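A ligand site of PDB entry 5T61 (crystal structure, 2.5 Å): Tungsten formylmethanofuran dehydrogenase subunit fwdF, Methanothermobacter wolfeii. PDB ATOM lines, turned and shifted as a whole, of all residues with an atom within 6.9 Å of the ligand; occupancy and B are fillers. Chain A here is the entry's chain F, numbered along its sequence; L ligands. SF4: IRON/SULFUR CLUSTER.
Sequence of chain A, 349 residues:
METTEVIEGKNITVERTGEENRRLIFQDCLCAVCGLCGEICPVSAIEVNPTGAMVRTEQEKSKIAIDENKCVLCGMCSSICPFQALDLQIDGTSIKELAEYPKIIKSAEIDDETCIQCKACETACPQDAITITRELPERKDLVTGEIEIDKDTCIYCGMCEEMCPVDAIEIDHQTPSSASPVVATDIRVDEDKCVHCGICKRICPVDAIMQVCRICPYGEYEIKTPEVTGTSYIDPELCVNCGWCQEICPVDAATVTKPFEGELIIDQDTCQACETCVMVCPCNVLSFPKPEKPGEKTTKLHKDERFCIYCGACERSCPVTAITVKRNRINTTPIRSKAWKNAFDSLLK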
ATOM      1  N   CYS A  34     -18.451   6.265 -24.738  1.00  0.00           N
ATOM      2  CA  CYS A  34     -19.251   6.385 -25.951  1.00  0.00           C
ATOM      3  C   CYS A  34     -18.514   5.839 -27.173  1.00  0.00           C
ATOM      4  O   CYS A  34     -19.165   5.490 -28.163  1.00  0.00           O
ATOM      5  CB  CYS A  34     -19.680   7.831 -26.205  1.00  0.00           C
ATOM      6  SG  CYS A  34     -18.475   8.919 -26.986  1.00  0.00           S
ATOM      7  N   PHE A  83     -17.279  14.522 -23.172  1.00  0.00           N
ATOM      8  CA  PHE A  83     -17.336  14.371 -21.723  1.00  0.00           C
ATOM      9  C   PHE A  83     -16.092  14.904 -21.010  1.00  0.00           C
ATOM     10  O   PHE A  83     -15.938  14.673 -19.812  1.00  0.00           O
ATOM     11  CB  PHE A  83     -17.589  12.906 -21.372  1.00  0.00           C
ATOM     12  CG  PHE A  83     -18.816  12.344 -22.041  1.00  0.00           C
ATOM     13  CD1 PHE A  83     -20.060  12.498 -21.453  1.00  0.00           C
ATOM     14  CD2 PHE A  83     -18.722  11.684 -23.255  1.00  0.00           C
ATOM     15  CE1 PHE A  83     -21.192  11.995 -22.063  1.00  0.00           C
ATOM     16  CE2 PHE A  83     -19.852  11.186 -23.873  1.00  0.00           C
ATOM     17  CZ  PHE A  83     -21.091  11.347 -23.280  1.00  0.00           C
ATOM     18  N   LEU A 264     -32.021   9.727 -33.451  1.00  0.00           N
ATOM     19  CA  LEU A 264     -32.113   8.476 -32.700  1.00  0.00           C
ATOM     20  C   LEU A 264     -33.206   7.624 -33.344  1.00  0.00           C
ATOM     21  O   LEU A 264     -34.296   8.125 -33.634  1.00  0.00           O
ATOM     22  CB  LEU A 264     -32.436   8.731 -31.220  1.00  0.00           C
ATOM     23  CG  LEU A 264     -31.328   8.684 -30.173  1.00  0.00           C
ATOM     24  CD1 LEU A 264     -31.930   8.709 -28.762  1.00  0.00           C
ATOM     25  CD2 LEU A 264     -30.428   7.475 -30.345  1.00  0.00           C
ATOM     26  N   CYS A 277     -29.085   0.385 -22.120  1.00  0.00           N
ATOM     27  CA  CYS A 277     -28.962   1.705 -22.718  1.00  0.00           C
ATOM     28  C   CYS A 277     -29.503   2.777 -21.797  1.00  0.00           C
ATOM     29  O   CYS A 277     -28.967   3.894 -21.752  1.00  0.00           O
ATOM     30  CB  CYS A 277     -29.712   1.758 -24.050  1.00  0.00           C
ATOM     31  SG  CYS A 277     -31.498   2.041 -23.823  1.00  0.00           S
ATOM     32  N   VAL A 280     -26.888   3.403 -19.377  1.00  0.00           N
ATOM     33  CA  VAL A 280     -25.681   3.906 -20.024  1.00  0.00           C
ATOM     34  C   VAL A 280     -25.823   5.390 -20.350  1.00  0.00           C
ATOM     35  O   VAL A 280     -24.883   6.174 -20.179  1.00  0.00           O
ATOM     36  CB  VAL A 280     -25.376   3.077 -21.282  1.00  0.00           C
ATOM     37  CG1 VAL A 280     -24.570   3.898 -22.299  1.00  0.00           C
ATOM     38  CG2 VAL A 280     -24.637   1.793 -20.915  1.00  0.00           C
ATOM     39  N   CYS A 281     -27.011   5.811 -20.808  1.00  0.00           N
ATOM     40  CA  CYS A 281     -27.264   7.163 -21.276  1.00  0.00           C
ATOM     41  C   CYS A 281     -26.861   8.208 -20.239  1.00  0.00           C
ATOM     42  O   CYS A 281     -27.496   8.325 -19.188  1.00  0.00           O
ATOM     43  CB  CYS A 281     -28.749   7.339 -21.601  1.00  0.00           C
ATOM     44  SG  CYS A 281     -29.237   9.056 -21.812  1.00  0.00           S
ATOM     45  N   PRO A 282     -25.805   8.987 -20.507  1.00  0.00           N
ATOM     46  CA  PRO A 282     -25.372  10.021 -19.567  1.00  0.00           C
ATOM     47  C   PRO A 282     -26.262  11.258 -19.567  1.00  0.00           C
ATOM     48  O   PRO A 282     -26.075  12.120 -18.691  1.00  0.00           O
ATOM     49  CB  PRO A 282     -23.957  10.362 -20.041  1.00  0.00           C
ATOM     50  CG  PRO A 282     -24.006  10.093 -21.514  1.00  0.00           C
ATOM     51  CD  PRO A 282     -24.967   8.964 -21.724  1.00  0.00           C
ATOM     52  N   CYS A 283     -27.191  11.368 -20.506  1.00  0.00           N
ATOM     53  CA  CYS A 283     -28.059  12.533 -20.630  1.00  0.00           C
ATOM     54  C   CYS A 283     -29.502  12.270 -20.217  1.00  0.00           C
ATOM     55  O   CYS A 283     -30.339  13.169 -20.361  1.00  0.00           O
ATOM     56  CB  CYS A 283     -28.032  13.054 -22.066  1.00  0.00           C
ATOM     57  SG  CYS A 283     -26.414  13.571 -22.656  1.00  0.00           S
ATOM     58  N   ASN A 284     -29.821  11.078 -19.716  1.00  0.00           N
ATOM     59  CA  ASN A 284     -31.181  10.715 -19.309  1.00  0.00           C
ATOM     60  C   ASN A 284     -32.171  10.850 -20.464  1.00  0.00           C
ATOM     61  O   ASN A 284     -33.264  11.384 -20.309  1.00  0.00           O
ATOM     62  CB  ASN A 284     -31.678  11.543 -18.109  1.00  0.00           C
ATOM     63  CG  ASN A 284     -31.260  10.942 -16.789  1.00  0.00           C
ATOM     64  OD1 ASN A 284     -30.217  11.294 -16.236  1.00  0.00           O
ATOM     65  ND2 ASN A 284     -32.077  10.024 -16.271  1.00  0.00           N
ATOM     66  N   VAL A 285     -31.774  10.346 -21.629  1.00  0.00           N
ATOM     67  CA  VAL A 285     -32.652  10.431 -22.790  1.00  0.00           C
ATOM     68  C   VAL A 285     -33.692   9.311 -22.767  1.00  0.00           C
ATOM     69  O   VAL A 285     -34.837   9.507 -23.193  1.00  0.00           O
ATOM     70  CB  VAL A 285     -31.820  10.407 -24.079  1.00  0.00           C
ATOM     71  CG1 VAL A 285     -32.713  10.495 -25.311  1.00  0.00           C
ATOM     72  CG2 VAL A 285     -30.787  11.517 -24.062  1.00  0.00           C
ATOM     73  N   LEU A 286     -33.332   8.148 -22.251  1.00  0.00           N
ATOM     74  CA  LEU A 286     -34.107   6.926 -22.402  1.00  0.00           C
ATOM     75  C   LEU A 286     -34.753   6.540 -21.074  1.00  0.00           C
ATOM     76  O   LEU A 286     -34.152   6.730 -20.010  1.00  0.00           O
ATOM     77  CB  LEU A 286     -33.219   5.800 -22.925  1.00  0.00           C
ATOM     78  CG  LEU A 286     -32.456   6.237 -24.184  1.00  0.00           C
ATOM     79  CD1 LEU A 286     -31.320   5.301 -24.525  1.00  0.00           C
ATOM     80  CD2 LEU A 286     -33.410   6.358 -25.356  1.00  0.00           C
ATOM     81  N   GLU A 305     -35.464  13.216 -27.636  1.00  0.00           N
ATOM     82  CA  GLU A 305     -34.227  13.687 -28.228  1.00  0.00           C
ATOM     83  C   GLU A 305     -33.887  15.126 -27.864  1.00  0.00           C
ATOM     84  O   GLU A 305     -32.808  15.596 -28.226  1.00  0.00           O
ATOM     85  CB  GLU A 305     -34.246  13.528 -29.747  1.00  0.00           C
ATOM     86  CG  GLU A 305     -34.092  12.097 -30.238  1.00  0.00           C
ATOM     87  CD  GLU A 305     -33.782  12.027 -31.723  1.00  0.00           C
ATOM     88  OE1 GLU A 305     -32.639  11.681 -32.075  1.00  0.00           O
ATOM     89  OE2 GLU A 305     -34.687  12.326 -32.530  1.00  0.00           O
ATOM     90  N   PHE A 307     -32.948  16.019 -25.108  1.00  0.00           N
ATOM     91  CA  PHE A 307     -31.838  15.880 -24.177  1.00  0.00           C
ATOM     92  C   PHE A 307     -30.678  15.095 -24.776  1.00  0.00           C
ATOM     93  O   PHE A 307     -29.682  14.861 -24.095  1.00  0.00           O
ATOM     94  CB  PHE A 307     -32.314  15.215 -22.895  1.00  0.00           C
ATOM     95  CG  PHE A 307     -33.605  15.801 -22.364  1.00  0.00           C
ATOM     96  CD1 PHE A 307     -33.685  17.131 -22.010  1.00  0.00           C
ATOM     97  CD2 PHE A 307     -34.739  15.006 -22.233  1.00  0.00           C
ATOM     98  CE1 PHE A 307     -34.871  17.675 -21.528  1.00  0.00           C
ATOM     99  CE2 PHE A 307     -35.918  15.540 -21.744  1.00  0.00           C
ATOM    100  CZ  PHE A 307     -35.984  16.872 -21.388  1.00  0.00           C
ATOM    101  N   CYS A 308     -30.782  14.702 -26.037  1.00  0.00           N
ATOM    102  CA  CYS A 308     -29.825  13.832 -26.688  1.00  0.00           C
ATOM    103  C   CYS A 308     -28.659  14.627 -27.277  1.00  0.00           C
ATOM    104  O   CYS A 308     -28.860  15.728 -27.812  1.00  0.00           O
ATOM    105  CB  CYS A 308     -30.564  13.042 -27.773  1.00  0.00           C
ATOM    106  SG  CYS A 308     -29.593  12.030 -28.866  1.00  0.00           S
ATOM    107  N   ILE A 309     -27.446  14.086 -27.163  1.00  0.00           N
ATOM    108  CA  ILE A 309     -26.258  14.710 -27.737  1.00  0.00           C
ATOM    109  C   ILE A 309     -25.583  13.843 -28.786  1.00  0.00           C
ATOM    110  O   ILE A 309     -24.525  14.238 -29.304  1.00  0.00           O
ATOM    111  CB  ILE A 309     -25.232  15.094 -26.645  1.00  0.00           C
ATOM    112  CG1 ILE A 309     -24.616  13.853 -26.006  1.00  0.00           C
ATOM    113  CG2 ILE A 309     -25.876  15.999 -25.604  1.00  0.00           C
ATOM    114  CD1 ILE A 309     -23.472  14.158 -25.069  1.00  0.00           C
ATOM    115  N   TYR A 310     -26.142  12.677 -29.101  1.00  0.00           N
ATOM    116  CA  TYR A 310     -25.677  11.836 -30.207  1.00  0.00           C
ATOM    117  C   TYR A 310     -24.230  11.385 -30.021  1.00  0.00           C
ATOM    118  O   TYR A 310     -23.457  11.324 -30.973  1.00  0.00           O
ATOM    119  CB  TYR A 310     -25.872  12.565 -31.539  1.00  0.00           C
ATOM    120  CG  TYR A 310     -27.264  13.159 -31.641  1.00  0.00           C
ATOM    121  CD1 TYR A 310     -28.356  12.357 -31.911  1.00  0.00           C
ATOM    122  CD2 TYR A 310     -27.477  14.508 -31.398  1.00  0.00           C
ATOM    123  CE1 TYR A 310     -29.635  12.887 -31.981  1.00  0.00           C
ATOM    124  CE2 TYR A 310     -28.746  15.052 -31.458  1.00  0.00           C
ATOM    125  CZ  TYR A 310     -29.822  14.227 -31.752  1.00  0.00           C
ATOM    126  OH  TYR A 310     -31.093  14.747 -31.815  1.00  0.00           O
ATOM    127  N   CYS A 311     -23.868  11.063 -28.771  1.00  0.00           N
ATOM    128  CA  CYS A 311     -22.541  10.502 -28.526  1.00  0.00           C
ATOM    129  C   CYS A 311     -22.459   9.053 -28.977  1.00  0.00           C
ATOM    130  O   CYS A 311     -21.347   8.567 -29.219  1.00  0.00           O
ATOM    131  CB  CYS A 311     -22.161  10.611 -27.054  1.00  0.00           C
ATOM    132  SG  CYS A 311     -22.883   9.371 -25.957  1.00  0.00           S
ATOM    133  N   GLY A 312     -23.581   8.356 -29.079  1.00  0.00           N
ATOM    134  CA  GLY A 312     -23.580   6.991 -29.582  1.00  0.00           C
ATOM    135  C   GLY A 312     -23.373   5.916 -28.545  1.00  0.00           C
ATOM    136  O   GLY A 312     -23.190   4.751 -28.915  1.00  0.00           O
ATOM    137  N   ALA A 313     -23.392   6.266 -27.255  1.00  0.00           N
ATOM    138  CA  ALA A 313     -23.088   5.280 -26.222  1.00  0.00           C
ATOM    139  C   ALA A 313     -24.182   4.227 -26.093  1.00  0.00           C
ATOM    140  O   ALA A 313     -23.886   3.059 -25.789  1.00  0.00           O
ATOM    141  CB  ALA A 313     -22.862   5.976 -24.889  1.00  0.00           C
ATOM    142  N   CYS A 314     -25.444   4.601 -26.305  1.00  0.00           N
ATOM    143  CA  CYS A 314     -26.530   3.639 -26.212  1.00  0.00           C
ATOM    144  C   CYS A 314     -26.424   2.576 -27.296  1.00  0.00           C
ATOM    145  O   CYS A 314     -26.455   1.381 -27.012  1.00  0.00           O
ATOM    146  CB  CYS A 314     -27.871   4.344 -26.322  1.00  0.00           C
ATOM    147  SG  CYS A 314     -28.149   4.950 -28.001  1.00  0.00           S
ATOM    148  N   GLU A 315     -26.327   3.023 -28.556  1.00  0.00           N
ATOM    149  CA  GLU A 315     -26.148   2.102 -29.674  1.00  0.00           C
ATOM    150  C   GLU A 315     -24.998   1.144 -29.411  1.00  0.00           C
ATOM    151  O   GLU A 315     -25.120  -0.065 -29.620  1.00  0.00           O
ATOM    152  CB  GLU A 315     -25.872   2.892 -30.961  1.00  0.00           C
ATOM    153  CG  GLU A 315     -25.578   1.997 -32.155  1.00  0.00           C
ATOM    154  CD  GLU A 315     -25.412   2.765 -33.456  1.00  0.00           C
ATOM    155  OE1 GLU A 315     -25.250   2.116 -34.514  1.00  0.00           O
ATOM    156  OE2 GLU A 315     -25.540   4.007 -33.435  1.00  0.00           O
ATOM    157  N   ILE A 323     -31.192   0.007 -31.125  1.00  0.00           N
ATOM    158  CA  ILE A 323     -31.175   1.466 -31.118  1.00  0.00           C
ATOM    159  C   ILE A 323     -29.933   1.916 -31.887  1.00  0.00           C
ATOM    160  O   ILE A 323     -28.819   1.428 -31.622  1.00  0.00           O
ATOM    161  CB  ILE A 323     -31.198   2.010 -29.672  1.00  0.00           C
ATOM    162  CG1 ILE A 323     -31.023   3.523 -29.624  1.00  0.00           C
ATOM    163  CG2 ILE A 323     -30.163   1.295 -28.800  1.00  0.00           C
ATOM    164  CD1 ILE A 323     -31.444   4.125 -28.307  1.00  0.00           C
ATOM    165  N   VAL A 325     -27.846   5.403 -33.868  1.00  0.00           N
ATOM    166  CA  VAL A 325     -27.623   6.846 -33.752  1.00  0.00           C
ATOM    167  C   VAL A 325     -27.115   7.346 -35.096  1.00  0.00           C
ATOM    168  O   VAL A 325     -26.166   6.793 -35.659  1.00  0.00           O
ATOM    169  CB  VAL A 325     -26.606   7.167 -32.642  1.00  0.00           C
ATOM    170  CG1 VAL A 325     -26.329   8.665 -32.579  1.00  0.00           C
ATOM    171  CG2 VAL A 325     -27.100   6.632 -31.305  1.00  0.00           C
HETATM  172 FE1  SF4 L   1     -28.498  10.442 -27.168  1.00  0.00          FE
HETATM  173 FE2  SF4 L   1     -28.178   9.162 -24.235  1.00  0.00          FE
HETATM  174 FE3  SF4 L   1     -25.570   9.623 -26.115  1.00  0.00          FE
HETATM  175 FE4  SF4 L   1     -27.715   7.331 -26.900  1.00  0.00          FE
HETATM  176  S1  SF4 L   1     -26.683   8.082 -25.237  1.00  0.00           S
HETATM  177  S2  SF4 L   1     -26.930   9.139 -27.627  1.00  0.00           S
HETATM  178  S3  SF4 L   1     -29.035   8.734 -26.091  1.00  0.00           S
HETATM  179  S4  SF4 L   1     -27.289  10.606 -25.470  1.00  0.00           S
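The backbone NH of Tyr 310 lies close to the side-chain sulfur of Cys 308 (3.5 Å). The side-chain sulfur (SG) of Cys 281 lies close to the backbone NH (N) of Val 285 (2.9 Å). The side-chain sulfur (SG) of Cys 281 lies close to the backbone NH (N) of Cys 283 (3.4 Å). The backbone NH (N) of Asn 284 sits close to the side-chain sulfur (SG) of Cys 281, 3.0 Å away. SG of Cys 311 lies close to N of Ala 313 (3.4 Å). O of Cys 311 lies close to SG of Cys 34 (3.7 Å). OE1 of Glu 305 sits close to OH of Tyr 310, at 3.4 Å. OE1 of Glu 305 lies within hydrogen-bond range of N of Leu 264, at 2.5 Å.
Leu 264 touches the ligand. Val 285 touches the ligand (CG2 to FE2, 3.5 Å). N of Ile 309 touches FE1 of the ligand, 3.8 Å away. N of Tyr 310 touches FE1 of the ligand (3.8 Å). The nearest printed residue that does not touch the ligand is Pro 282 (4.01 Å).
SG of Cys 308 binds FE1 of the ligand. An iron atom (FE2) of the ligand is bound by the side-chain sulfur (SG) of Cys 281 (2.6 Å). The side-chain sulfur of Cys 314 is bound to an iron atom (FE4) of the ligand (2.7 Å). A sulfur (S2) of the ligand sits close to the backbone NH of Cys 311. An iron atom (FE3) of the ligand is bound by the side-chain sulfur of Cys 311. N of Gly 312 sits close to S2 of the ligand (3.7 Å).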
